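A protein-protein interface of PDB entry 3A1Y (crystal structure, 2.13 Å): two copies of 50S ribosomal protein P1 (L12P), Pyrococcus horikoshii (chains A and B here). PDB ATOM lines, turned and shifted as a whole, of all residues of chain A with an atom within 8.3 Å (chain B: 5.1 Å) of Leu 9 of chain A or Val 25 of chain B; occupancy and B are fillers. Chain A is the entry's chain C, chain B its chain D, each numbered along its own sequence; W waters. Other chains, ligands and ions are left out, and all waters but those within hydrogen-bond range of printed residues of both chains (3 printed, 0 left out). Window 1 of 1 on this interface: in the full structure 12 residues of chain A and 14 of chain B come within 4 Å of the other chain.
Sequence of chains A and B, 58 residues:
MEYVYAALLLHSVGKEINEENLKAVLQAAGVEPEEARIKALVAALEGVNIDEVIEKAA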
ATOM      1  N   GLU A   2      35.129   4.537 -30.710  1.00  0.00           N
ATOM      2  CA  GLU A   2      33.748   4.975 -30.864  1.00  0.00           C
ATOM      3  C   GLU A   2      32.835   3.832 -30.430  1.00  0.00           C
ATOM      4  O   GLU A   2      31.816   4.062 -29.764  1.00  0.00           O
ATOM      5  CB  GLU A   2      33.465   5.423 -32.311  1.00  0.00           C
ATOM      6  CG  GLU A   2      33.058   4.316 -33.284  1.00  0.00           C
ATOM      7  CD  GLU A   2      33.498   4.567 -34.733  1.00  0.00           C
ATOM      8  OE1 GLU A   2      34.680   4.905 -34.952  1.00  0.00           O
ATOM      9  OE2 GLU A   2      32.671   4.392 -35.660  1.00  0.00           O
ATOM     10  N   TYR A   3      33.236   2.603 -30.767  1.00  0.00           N
ATOM     11  CA  TYR A   3      32.537   1.394 -30.311  1.00  0.00           C
ATOM     12  C   TYR A   3      32.600   1.232 -28.788  1.00  0.00           C
ATOM     13  O   TYR A   3      31.592   0.949 -28.153  1.00  0.00           O
ATOM     14  CB  TYR A   3      33.060   0.143 -31.033  1.00  0.00           C
ATOM     15  CG  TYR A   3      32.832   0.232 -32.522  1.00  0.00           C
ATOM     16  CD1 TYR A   3      31.594  -0.106 -33.072  1.00  0.00           C
ATOM     17  CD2 TYR A   3      33.832   0.700 -33.377  1.00  0.00           C
ATOM     18  CE1 TYR A   3      31.351  -0.003 -34.431  1.00  0.00           C
ATOM     19  CE2 TYR A   3      33.604   0.807 -34.756  1.00  0.00           C
ATOM     20  CZ  TYR A   3      32.348   0.458 -35.266  1.00  0.00           C
ATOM     21  OH  TYR A   3      32.094   0.550 -36.608  1.00  0.00           O
ATOM     22  N   VAL A   4      33.786   1.433 -28.214  1.00  0.00           N
ATOM     23  CA  VAL A   4      33.967   1.343 -26.763  1.00  0.00           C
ATOM     24  C   VAL A   4      33.170   2.406 -25.987  1.00  0.00           C
ATOM     25  O   VAL A   4      32.557   2.103 -24.961  1.00  0.00           O
ATOM     26  CB  VAL A   4      35.458   1.401 -26.415  1.00  0.00           C
ATOM     27  CG1 VAL A   4      35.682   1.229 -24.924  1.00  0.00           C
ATOM     28  CG2 VAL A   4      36.204   0.331 -27.226  1.00  0.00           C
ATOM     29  N   TYR A   5      33.160   3.641 -26.478  1.00  0.00           N
ATOM     30  CA  TYR A   5      32.385   4.705 -25.813  1.00  0.00           C
ATOM     31  C   TYR A   5      30.889   4.404 -25.836  1.00  0.00           C
ATOM     32  O   TYR A   5      30.202   4.591 -24.838  1.00  0.00           O
ATOM     33  CB  TYR A   5      32.662   6.070 -26.432  1.00  0.00           C
ATOM     34  CG  TYR A   5      34.064   6.571 -26.211  1.00  0.00           C
ATOM     35  CD1 TYR A   5      34.642   6.589 -24.935  1.00  0.00           C
ATOM     36  CD2 TYR A   5      34.803   7.067 -27.270  1.00  0.00           C
ATOM     37  CE1 TYR A   5      35.937   7.068 -24.750  1.00  0.00           C
ATOM     38  CE2 TYR A   5      36.082   7.546 -27.092  1.00  0.00           C
ATOM     39  CZ  TYR A   5      36.644   7.546 -25.834  1.00  0.00           C
ATOM     40  OH  TYR A   5      37.930   8.028 -25.681  1.00  0.00           O
ATOM     41  N   ALA A   6      30.404   3.915 -26.973  1.00  0.00           N
ATOM     42  CA  ALA A   6      29.025   3.421 -27.088  1.00  0.00           C
ATOM     43  C   ALA A   6      28.709   2.356 -26.027  1.00  0.00           C
ATOM     44  O   ALA A   6      27.675   2.437 -25.360  1.00  0.00           O
ATOM     45  CB  ALA A   6      28.747   2.899 -28.498  1.00  0.00           C
ATOM     46  N   ALA A   7      29.628   1.398 -25.841  1.00  0.00           N
ATOM     47  CA  ALA A   7      29.473   0.364 -24.817  1.00  0.00           C
ATOM     48  C   ALA A   7      29.400   0.917 -23.399  1.00  0.00           C
ATOM     49  O   ALA A   7      28.496   0.566 -22.647  1.00  0.00           O
ATOM     50  CB  ALA A   7      30.582  -0.662 -24.918  1.00  0.00           C
ATOM     51  N   LEU A   8      30.348   1.782 -23.039  1.00  0.00           N
ATOM     52  CA  LEU A   8      30.414   2.311 -21.682  1.00  0.00           C
ATOM     53  C   LEU A   8      29.247   3.239 -21.384  1.00  0.00           C
ATOM     54  O   LEU A   8      28.772   3.290 -20.246  1.00  0.00           O
ATOM     55  CB  LEU A   8      31.742   3.014 -21.425  1.00  0.00           C
ATOM     56  CG  LEU A   8      32.909   2.059 -21.116  1.00  0.00           C
ATOM     57  CD1 LEU A   8      34.110   2.855 -20.715  1.00  0.00           C
ATOM     58  CD2 LEU A   8      32.541   1.066 -19.999  1.00  0.00           C
ATOM     59  N   LEU A   9      28.791   3.967 -22.407  1.00  0.00           N
ATOM     60  CA  LEU A   9      27.552   4.738 -22.289  1.00  0.00           C
ATOM     61  C   LEU A   9      26.408   3.820 -21.862  1.00  0.00           C
ATOM     62  O   LEU A   9      25.754   4.072 -20.854  1.00  0.00           O
ATOM     63  CB  LEU A   9      27.212   5.468 -23.590  1.00  0.00           C
ATOM     64  CG  LEU A   9      25.810   6.074 -23.672  1.00  0.00           C
ATOM     65  CD1 LEU A   9      25.622   7.119 -22.593  1.00  0.00           C
ATOM     66  CD2 LEU A   9      25.567   6.672 -25.026  1.00  0.00           C
ATOM     67  N   LEU A  10      26.213   2.735 -22.611  1.00  0.00           N
ATOM     68  CA  LEU A  10      25.219   1.717 -22.283  1.00  0.00           C
ATOM     69  C   LEU A  10      25.370   1.208 -20.851  1.00  0.00           C
ATOM     70  O   LEU A  10      24.409   1.190 -20.077  1.00  0.00           O
ATOM     71  CB  LEU A  10      25.319   0.557 -23.278  1.00  0.00           C
ATOM     72  CG  LEU A  10      24.345   0.381 -24.450  1.00  0.00           C
ATOM     73  CD1 LEU A  10      23.304   1.492 -24.658  1.00  0.00           C
ATOM     74  CD2 LEU A  10      25.115   0.074 -25.728  1.00  0.00           C
ATOM     75  N   HIS A  11      26.585   0.807 -20.499  1.00  0.00           N
ATOM     76  CA  HIS A  11      26.869   0.344 -19.149  1.00  0.00           C
ATOM     77  C   HIS A  11      26.550   1.414 -18.086  1.00  0.00           C
ATOM     78  O   HIS A  11      25.963   1.110 -17.030  1.00  0.00           O
ATOM     79  CB  HIS A  11      28.329  -0.120 -19.041  1.00  0.00           C
ATOM     80  CG  HIS A  11      28.705  -0.601 -17.674  1.00  0.00           C
ATOM     81  ND1 HIS A  11      28.388  -1.862 -17.216  1.00  0.00           N
ATOM     82  CD2 HIS A  11      29.348   0.021 -16.656  1.00  0.00           C
ATOM     83  CE1 HIS A  11      28.819  -1.996 -15.973  1.00  0.00           C
ATOM     84  NE2 HIS A  11      29.414  -0.871 -15.613  1.00  0.00           N
ATOM     85  N   SER A  12      26.922   2.662 -18.363  1.00  0.00           N
ATOM     86  CA  SER A  12      26.720   3.724 -17.377  1.00  0.00           C
ATOM     87  C   SER A  12      25.233   4.008 -17.103  1.00  0.00           C
ATOM     88  O   SER A  12      24.878   4.454 -16.013  1.00  0.00           O
ATOM     89  CB  SER A  12      27.438   4.999 -17.794  1.00  0.00           C
ATOM     90  OG  SER A  12      26.720   5.665 -18.819  1.00  0.00           O
ATOM     91  N   VAL A  13      24.368   3.751 -18.084  1.00  0.00           N
ATOM     92  CA  VAL A  13      22.919   3.910 -17.859  1.00  0.00           C
ATOM     93  C   VAL A  13      22.184   2.583 -17.602  1.00  0.00           C
ATOM     94  O   VAL A  13      20.957   2.538 -17.609  1.00  0.00           O
ATOM     95  CB  VAL A  13      22.215   4.764 -18.955  1.00  0.00           C
ATOM     96  CG1 VAL A  13      22.689   6.214 -18.882  1.00  0.00           C
ATOM     97  CG2 VAL A  13      22.419   4.172 -20.353  1.00  0.00           C
ATOM     98  N   GLY A  14      22.949   1.522 -17.349  1.00  0.00           N
ATOM     99  CA  GLY A  14      22.392   0.234 -16.928  1.00  0.00           C
ATOM    100  C   GLY A  14      21.769  -0.578 -18.046  1.00  0.00           C
ATOM    101  O   GLY A  14      20.948  -1.463 -17.801  1.00  0.00           O
ATOM    102  N   LYS A  15      22.171  -0.286 -19.276  1.00  0.00           N
ATOM    103  CA  LYS A  15      21.627  -0.975 -20.434  1.00  0.00           C
ATOM    104  C   LYS A  15      22.598  -2.049 -20.928  1.00  0.00           C
ATOM    105  O   LYS A  15      23.829  -1.890 -20.866  1.00  0.00           O
ATOM    106  CB  LYS A  15      21.264   0.027 -21.537  1.00  0.00           C
ATOM    107  CG  LYS A  15      20.147   1.009 -21.148  1.00  0.00           C
ATOM    108  CD  LYS A  15      18.794   0.305 -21.019  1.00  0.00           C
ATOM    109  CE  LYS A  15      17.802   1.105 -20.176  1.00  0.00           C
ATOM    110  NZ  LYS A  15      16.703   1.727 -20.980  1.00  0.00           N
ATOM    111  N   GLU A  16      22.025  -3.151 -21.396  1.00  0.00           N
ATOM    112  CA  GLU A  16      22.795  -4.310 -21.800  1.00  0.00           C
ATOM    113  C   GLU A  16      23.639  -3.988 -23.027  1.00  0.00           C
ATOM    114  O   GLU A  16      23.146  -3.420 -24.006  1.00  0.00           O
ATOM    115  CB  GLU A  16      21.866  -5.495 -22.083  1.00  0.00           C
ATOM    116  CG  GLU A  16      22.270  -6.800 -21.386  1.00  0.00           C
ATOM    117  CD  GLU A  16      21.954  -6.788 -19.888  1.00  0.00           C
ATOM    118  OE1 GLU A  16      22.548  -5.969 -19.144  1.00  0.00           O
ATOM    119  OE2 GLU A  16      21.105  -7.601 -19.452  1.00  0.00           O
ATOM    120  N   ILE A  17      24.919  -4.331 -22.959  1.00  0.00           N
ATOM    121  CA  ILE A  17      25.795  -4.174 -24.106  1.00  0.00           C
ATOM    122  C   ILE A  17      25.558  -5.363 -25.031  1.00  0.00           C
ATOM    123  O   ILE A  17      26.127  -6.435 -24.851  1.00  0.00           O
ATOM    124  CB  ILE A  17      27.289  -4.035 -23.689  1.00  0.00           C
ATOM    125  CG1 ILE A  17      27.452  -2.868 -22.698  1.00  0.00           C
ATOM    126  CG2 ILE A  17      28.178  -3.851 -24.915  1.00  0.00           C
ATOM    127  CD1 ILE A  17      28.845  -2.715 -22.114  1.00  0.00           C
ATOM    128  N   ASN A  21      21.615  -2.518 -29.114  1.00  0.00           N
ATOM    129  CA  ASN A  21      21.763  -1.294 -28.332  1.00  0.00           C
ATOM    130  C   ASN A  21      22.950  -0.482 -28.850  1.00  0.00           C
ATOM    131  O   ASN A  21      22.843   0.736 -29.067  1.00  0.00           O
ATOM    132  CB  ASN A  21      21.913  -1.628 -26.843  1.00  0.00           C
ATOM    133  CG  ASN A  21      20.614  -2.177 -26.210  1.00  0.00           C
ATOM    134  OD1 ASN A  21      20.582  -2.485 -25.015  1.00  0.00           O
ATOM    135  ND2 ASN A  21      19.551  -2.286 -27.000  1.00  0.00           N
ATOM    136  N   LEU A  22      24.063  -1.182 -29.076  1.00  0.00           N
ATOM    137  CA  LEU A  22      25.289  -0.602 -29.633  1.00  0.00           C
ATOM    138  C   LEU A  22      25.006   0.102 -30.959  1.00  0.00           C
ATOM    139  O   LEU A  22      25.345   1.276 -31.127  1.00  0.00           O
ATOM    140  CB  LEU A  22      26.353  -1.694 -29.829  1.00  0.00           C
ATOM    141  CG  LEU A  22      27.565  -1.888 -28.904  1.00  0.00           C
ATOM    142  CD1 LEU A  22      27.290  -1.645 -27.446  1.00  0.00           C
ATOM    143  CD2 LEU A  22      28.144  -3.261 -29.081  1.00  0.00           C
ATOM    144  N   ALA A  24      22.160   1.249 -32.286  1.00  0.00           N
ATOM    145  CA  ALA A  24      21.266   2.416 -32.159  1.00  0.00           C
ATOM    146  C   ALA A  24      21.998   3.681 -31.695  1.00  0.00           C
ATOM    147  O   ALA A  24      21.835   4.762 -32.279  1.00  0.00           O
ATOM    148  CB  ALA A  24      20.111   2.100 -31.211  1.00  0.00           C
ATOM    149  N   VAL A  25      22.801   3.521 -30.644  1.00  0.00           N
ATOM    150  CA  VAL A  25      23.631   4.590 -30.085  1.00  0.00           C
ATOM    151  C   VAL A  25      24.583   5.149 -31.154  1.00  0.00           C
ATOM    152  O   VAL A  25      24.675   6.373 -31.326  1.00  0.00           O
ATOM    153  CB  VAL A  25      24.388   4.085 -28.819  1.00  0.00           C
ATOM    154  CG1 VAL A  25      25.578   4.978 -28.453  1.00  0.00           C
ATOM    155  CG2 VAL A  25      23.428   3.968 -27.631  1.00  0.00           C
ATOM    156  N   LEU A  26      25.243   4.249 -31.894  1.00  0.00           N
ATOM    157  CA  LEU A  26      26.205   4.635 -32.938  1.00  0.00           C
ATOM    158  C   LEU A  26      25.525   5.372 -34.089  1.00  0.00           C
ATOM    159  O   LEU A  26      26.042   6.368 -34.572  1.00  0.00           O
ATOM    160  CB  LEU A  26      26.982   3.424 -33.491  1.00  0.00           C
ATOM    161  CG  LEU A  26      28.343   2.923 -32.956  1.00  0.00           C
ATOM    162  CD1 LEU A  26      29.070   3.931 -32.082  1.00  0.00           C
ATOM    163  CD2 LEU A  26      28.245   1.552 -32.271  1.00  0.00           C
ATOM    164  N   GLN A  27      24.376   4.867 -34.532  1.00  0.00           N
ATOM    165  CA  GLN A  27      23.578   5.526 -35.572  1.00  0.00           C
ATOM    166  C   GLN A  27      23.033   6.907 -35.134  1.00  0.00           C
ATOM    167  O   GLN A  27      22.920   7.833 -35.947  1.00  0.00           O
ATOM    168  CB  GLN A  27      22.442   4.604 -36.025  1.00  0.00           C
ATOM    169  CG  GLN A  27      22.936   3.324 -36.708  1.00  0.00           C
ATOM    170  CD  GLN A  27      21.807   2.436 -37.188  1.00  0.00           C
ATOM    171  OE1 GLN A  27      20.938   2.040 -36.407  1.00  0.00           O
ATOM    172  NE2 GLN A  27      21.819   2.107 -38.481  1.00  0.00           N
ATOM    173  N   ALA A  28      22.692   7.031 -33.850  1.00  0.00           N
ATOM    174  CA  ALA A  28      22.327   8.323 -33.257  1.00  0.00           C
ATOM    175  C   ALA A  28      23.521   9.272 -33.225  1.00  0.00           C
ATOM    176  O   ALA A  28      23.356  10.483 -33.338  1.00  0.00           O
ATOM    177  CB  ALA A  28      21.773   8.139 -31.865  1.00  0.00           C
ATOM    178  N   ALA A  29      24.722   8.721 -33.084  1.00  0.00           N
ATOM    179  CA  ALA A  29      25.928   9.536 -33.191  1.00  0.00           C
ATOM    180  C   ALA A  29      26.171   9.954 -34.637  1.00  0.00           C
ATOM    181  O   ALA A  29      27.057  10.748 -34.912  1.00  0.00           O
ATOM    182  CB  ALA A  29      27.149   8.800 -32.619  1.00  0.00           C
ATOM    183  N   GLY A  30      25.391   9.407 -35.561  1.00  0.00           N
ATOM    184  CA  GLY A  30      25.441   9.833 -36.952  1.00  0.00           C
ATOM    185  C   GLY A  30      26.383   9.034 -37.822  1.00  0.00           C
ATOM    186  O   GLY A  30      26.728   9.473 -38.915  1.00  0.00           O
ATOM    187  N   ILE A  50      33.220  -4.975 -16.092  1.00  0.00           N
ATOM    188  CA  ILE A  50      33.510  -3.582 -16.367  1.00  0.00           C
ATOM    189  C   ILE A  50      33.732  -2.753 -15.097  1.00  0.00           C
ATOM    190  O   ILE A  50      34.720  -2.018 -14.995  1.00  0.00           O
ATOM    191  CB  ILE A  50      32.416  -2.949 -17.249  1.00  0.00           C
ATOM    192  CG1 ILE A  50      32.439  -3.582 -18.648  1.00  0.00           C
ATOM    193  CG2 ILE A  50      32.600  -1.429 -17.332  1.00  0.00           C
ATOM    194  CD1 ILE A  50      31.203  -3.275 -19.484  1.00  0.00           C
ATOM    195  N   GLU B   2      27.423   9.153 -18.083  1.00  0.00           N
ATOM    196  CA  GLU B   2      26.873   8.931 -19.405  1.00  0.00           C
ATOM    197  C   GLU B   2      27.053  10.113 -20.358  1.00  0.00           C
ATOM    198  O   GLU B   2      27.178   9.921 -21.565  1.00  0.00           O
ATOM    199  CB  GLU B   2      25.381   8.594 -19.256  1.00  0.00           C
ATOM    200  CG  GLU B   2      24.577   9.552 -18.379  1.00  0.00           C
ATOM    201  CD  GLU B   2      24.406   9.090 -16.912  1.00  0.00           C
ATOM    202  OE1 GLU B   2      25.408   8.672 -16.269  1.00  0.00           O
ATOM    203  OE2 GLU B   2      23.256   9.167 -16.399  1.00  0.00           O
ATOM    204  N   TYR B   5      30.732  10.067 -21.753  1.00  0.00           N
ATOM    205  CA  TYR B   5      30.846   8.968 -22.738  1.00  0.00           C
ATOM    206  C   TYR B   5      30.138   9.294 -24.072  1.00  0.00           C
ATOM    207  O   TYR B   5      30.665   8.995 -25.136  1.00  0.00           O
ATOM    208  CB  TYR B   5      30.324   7.639 -22.176  1.00  0.00           C
ATOM    209  CG  TYR B   5      31.141   7.042 -21.038  1.00  0.00           C
ATOM    210  CD1 TYR B   5      32.535   6.956 -21.107  1.00  0.00           C
ATOM    211  CD2 TYR B   5      30.502   6.525 -19.907  1.00  0.00           C
ATOM    212  CE1 TYR B   5      33.282   6.393 -20.061  1.00  0.00           C
ATOM    213  CE2 TYR B   5      31.230   5.958 -18.859  1.00  0.00           C
ATOM    214  CZ  TYR B   5      32.619   5.908 -18.938  1.00  0.00           C
ATOM    215  OH  TYR B   5      33.322   5.340 -17.897  1.00  0.00           O
ATOM    216  N   ALA B   6      28.970   9.931 -24.010  1.00  0.00           N
ATOM    217  CA  ALA B   6      28.332  10.484 -25.198  1.00  0.00           C
ATOM    218  C   ALA B   6      29.153  11.587 -25.880  1.00  0.00           C
ATOM    219  O   ALA B   6      29.240  11.610 -27.107  1.00  0.00           O
ATOM    220  CB  ALA B   6      26.927  10.997 -24.867  1.00  0.00           C
ATOM    221  N   LEU B   9      32.081   9.871 -27.478  1.00  0.00           N
ATOM    222  CA  LEU B   9      31.606   9.181 -28.684  1.00  0.00           C
ATOM    223  C   LEU B   9      31.521  10.154 -29.861  1.00  0.00           C
ATOM    224  O   LEU B   9      32.098   9.904 -30.912  1.00  0.00           O
ATOM    225  CB  LEU B   9      30.259   8.516 -28.439  1.00  0.00           C
ATOM    226  CG  LEU B   9      29.513   7.915 -29.639  1.00  0.00           C
ATOM    227  CD1 LEU B   9      30.403   6.950 -30.470  1.00  0.00           C
ATOM    228  CD2 LEU B   9      28.270   7.213 -29.156  1.00  0.00           C
ATOM    229  N   LEU B  10      30.781  11.246 -29.669  1.00  0.00           N
ATOM    230  CA  LEU B  10      30.623  12.317 -30.661  1.00  0.00           C
ATOM    231  C   LEU B  10      31.968  12.809 -31.179  1.00  0.00           C
ATOM    232  O   LEU B  10      32.193  12.887 -32.394  1.00  0.00           O
ATOM    233  CB  LEU B  10      29.844  13.488 -30.024  1.00  0.00           C
ATOM    234  CG  LEU B  10      28.405  13.858 -30.407  1.00  0.00           C
ATOM    235  CD1 LEU B  10      27.612  12.813 -31.237  1.00  0.00           C
ATOM    236  CD2 LEU B  10      27.589  14.384 -29.196  1.00  0.00           C
ATOM    237  N   ASN B  21      23.031  16.988 -30.423  1.00  0.00           N
ATOM    238  CA  ASN B  21      23.692  15.698 -30.665  1.00  0.00           C
ATOM    239  C   ASN B  21      23.773  14.856 -29.398  1.00  0.00           C
ATOM    240  O   ASN B  21      23.533  13.646 -29.434  1.00  0.00           O
ATOM    241  CB  ASN B  21      25.072  15.881 -31.322  1.00  0.00           C
ATOM    242  CG  ASN B  21      24.990  16.629 -32.650  1.00  0.00           C
ATOM    243  OD1 ASN B  21      23.926  16.721 -33.255  1.00  0.00           O
ATOM    244  ND2 ASN B  21      26.111  17.168 -33.101  1.00  0.00           N
ATOM    245  N   LEU B  22      24.080  15.505 -28.274  1.00  0.00           N
ATOM    246  CA  LEU B  22      24.126  14.808 -26.983  1.00  0.00           C
ATOM    247  C   LEU B  22      22.773  14.197 -26.640  1.00  0.00           C
ATOM    248  O   LEU B  22      22.701  13.025 -26.258  1.00  0.00           O
ATOM    249  CB  LEU B  22      24.601  15.728 -25.856  1.00  0.00           C
ATOM    250  CG  LEU B  22      26.113  15.919 -25.731  1.00  0.00           C
ATOM    251  CD1 LEU B  22      26.428  17.066 -24.746  1.00  0.00           C
ATOM    252  CD2 LEU B  22      26.805  14.621 -25.274  1.00  0.00           C
ATOM    253  N   LYS B  23      21.710  14.987 -26.792  1.00  0.00           N
ATOM    254  CA  LYS B  23      20.357  14.502 -26.541  1.00  0.00           C
ATOM    255  C   LYS B  23      20.033  13.267 -27.379  1.00  0.00           C
ATOM    256  O   LYS B  23      19.541  12.271 -26.845  1.00  0.00           O
ATOM    257  CB  LYS B  23      19.306  15.610 -26.758  1.00  0.00           C
ATOM    258  CG  LYS B  23      17.881  15.185 -26.441  1.00  0.00           C
ATOM    259  CD  LYS B  23      17.044  16.327 -25.838  1.00  0.00           C
ATOM    260  CE  LYS B  23      16.446  17.251 -26.887  1.00  0.00           C
ATOM    261  NZ  LYS B  23      15.446  18.210 -26.268  1.00  0.00           N
ATOM    262  N   ALA B  24      20.312  13.337 -28.680  1.00  0.00           N
ATOM    263  CA  ALA B  24      19.997  12.246 -29.594  1.00  0.00           C
ATOM    264  C   ALA B  24      20.689  10.943 -29.184  1.00  0.00           C
ATOM    265  O   ALA B  24      20.084   9.856 -29.238  1.00  0.00           O
ATOM    266  CB  ALA B  24      20.379  12.628 -31.025  1.00  0.00           C
ATOM    267  N   VAL B  25      21.953  11.058 -28.781  1.00  0.00           N
ATOM    268  CA  VAL B  25      22.752   9.896 -28.396  1.00  0.00           C
ATOM    269  C   VAL B  25      22.204   9.234 -27.117  1.00  0.00           C
ATOM    270  O   VAL B  25      22.061   8.005 -27.067  1.00  0.00           O
ATOM    271  CB  VAL B  25      24.272  10.254 -28.298  1.00  0.00           C
ATOM    272  CG1 VAL B  25      25.067   9.157 -27.609  1.00  0.00           C
ATOM    273  CG2 VAL B  25      24.835  10.511 -29.692  1.00  0.00           C
ATOM    274  N   LEU B  26      21.892  10.051 -26.104  1.00  0.00           N
ATOM    275  CA  LEU B  26      21.387   9.548 -24.828  1.00  0.00           C
ATOM    276  C   LEU B  26      20.009   8.927 -24.978  1.00  0.00           C
ATOM    277  O   LEU B  26      19.759   7.846 -24.440  1.00  0.00           O
ATOM    278  CB  LEU B  26      21.368  10.649 -23.749  1.00  0.00           C
ATOM    279  CG  LEU B  26      22.614  10.962 -22.887  1.00  0.00           C
ATOM    280  CD1 LEU B  26      23.323   9.725 -22.355  1.00  0.00           C
ATOM    281  CD2 LEU B  26      23.599  11.794 -23.640  1.00  0.00           C
ATOM    282  N   GLN B  27      19.124   9.597 -25.717  1.00  0.00           N
ATOM    283  CA  GLN B  27      17.828   9.022 -26.065  1.00  0.00           C
ATOM    284  C   GLN B  27      17.983   7.653 -26.739  1.00  0.00           C
ATOM    285  O   GLN B  27      17.235   6.726 -26.428  1.00  0.00           O
ATOM    286  CB  GLN B  27      17.001   9.987 -26.934  1.00  0.00           C
ATOM    287  CG  GLN B  27      16.479  11.195 -26.160  1.00  0.00           C
ATOM    288  CD  GLN B  27      15.759  12.229 -27.026  1.00  0.00           C
ATOM    289  OE1 GLN B  27      16.049  12.386 -28.221  1.00  0.00           O
ATOM    290  NE2 GLN B  27      14.818  12.958 -26.411  1.00  0.00           N
ATOM    291  N   ALA B  28      18.981   7.513 -27.620  1.00  0.00           N
ATOM    292  CA  ALA B  28      19.187   6.258 -28.346  1.00  0.00           C
ATOM    293  C   ALA B  28      19.633   5.143 -27.416  1.00  0.00           C
ATOM    294  O   ALA B  28      19.422   3.961 -27.704  1.00  0.00           O
ATOM    295  CB  ALA B  28      20.183   6.437 -29.460  1.00  0.00           C
ATOM    296  N   ALA B  29      20.245   5.533 -26.300  1.00  0.00           N
ATOM    297  CA  ALA B  29      20.662   4.598 -25.258  1.00  0.00           C
ATOM    298  C   ALA B  29      19.475   4.111 -24.417  1.00  0.00           C
ATOM    299  O   ALA B  29      19.619   3.195 -23.611  1.00  0.00           O
ATOM    300  CB  ALA B  29      21.720   5.249 -24.365  1.00  0.00           C
HETATM  301  O   HOH W   1      23.966  12.876 -32.584  1.00  0.00           O
HETATM  302  O   HOH W   2      19.676   0.588 -24.784  1.00  0.00           O
HETATM  303  O   HOH W   3      20.235   1.430 -27.228  1.00  0.00           O
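The backbone carbonyl oxygen of Leu 8 of chain A lies close to the side-chain hydroxyl of Ser 12 of chain A. O of Leu 9 of chain A lies within hydrogen-bond range of OG of Ser 12 of chain A, 2.8 Å away. The backbone carbonyl oxygen (O) of Leu 10 of chain A is in hydrogen-bond range of the backbone NH (N) of Lys 15 of chain A, at 2.8 Å.
Tyr 5 of chain A touches Tyr 5 of chain B. Leu 9 of chain B touches Tyr 5 of chain A. Leu 9 of chain A touches Val 25 of chain B. CD1 of Leu 9 of chain A touches CD1 of Leu 26 of chain B, 3.5 Å away. Glu 2 of chain B touches Val 13 of chain A (CB to CG1, 3.6 Å). Ala 29 of chain B touches Lys 15 of chain A. Val 25 of chain A touches Leu 9 of chain B. Val 25 of chain A touches Ala 29 of chain B (CG2 to CA, 3.7 Å). CB of Ala 28 of chain B touches CB of Ala 28 of chain A, 3.3 Å away. Ala 29 of chain A touches Val 25 of chain B (CA to CG2, 3.8 Å).
Of the printed residues of chain B, Leu 9 of chain A touches Glu 2, Tyr 5, Val 25 and Leu 26. Val 25 of chain B touches just these residues of chain A: Leu 9, Ala 28 and Ala 29. Ala 24 of chain B touches just one residue of chain A: Ala 28 (3.6 Å). Of the printed residues of chain A, Ala 28 of chain B touches Ala 24 (3.7 Å), Val 25 (3.96 Å) and Ala 28 (3.3 Å). Printed residues of chain B within 4 Å of Ser 12 of chain A: Glu 2. Printed residues of chain B within 4 Å of Tyr 5 of chain A: Tyr 5 (3.8 Å) and Leu 9 (3.9 Å). The nearest residue of chain A that does not touch Val 25 of chain B is Val 25 of chain A (4.3 Å). The nearest printed residue of chain B that does not touch Ala 24 of chain A is Ala 29 of chain B (6.0 Å).
Printed residues of chain B that touch a printed residue of chain A: Glu 2, Tyr 5, Leu 9, Ala 24, Val 25, Leu 26, Ala 28 and Ala 29. Along chain B the printed residues that touch a printed residue of chain A span positions 2 to 29. Among the printed residues, no Asp or Glu carboxylate lies within 4 Å of a Lys or Arg side-chain nitrogen of the other chain.
Tyr 5 of chain A touches Leu 9 of chain B, and with the chains exchanged Leu 9 of chain A touches Tyr 5 of chain B. Val 25 of chain A touches Ala 29 of chain B, and with the chains exchanged Ala 29 of chain A touches Val 25 of chain B. Ala 28 of chain B touches its own counterpart, Ala 28 of chain A. Ala 29 of chain A touches Leu 9 of chain B, but with the chains exchanged Leu 9 of chain A does not touch Ala 29 of chain B (4.2 Å). Of the 21 pairs that touch across the chains among the printed residues, 16 have their exchanged pair printed and touching as well.
Water W1 lies within hydrogen-bond range of the backbone carbonyl oxygen of Ala 28 of chain A (2.6 Å) and the backbone carbonyl oxygen of Asn 21 of chain B (3.3 Å). Water W3 lies within hydrogen-bond range of O of Ala 28 of chain B and O of Asn 21 of chain A. Water W2 lies within hydrogen-bond range of O of Ala 29 of chain B and OD1 of Asn 21 of chain A.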
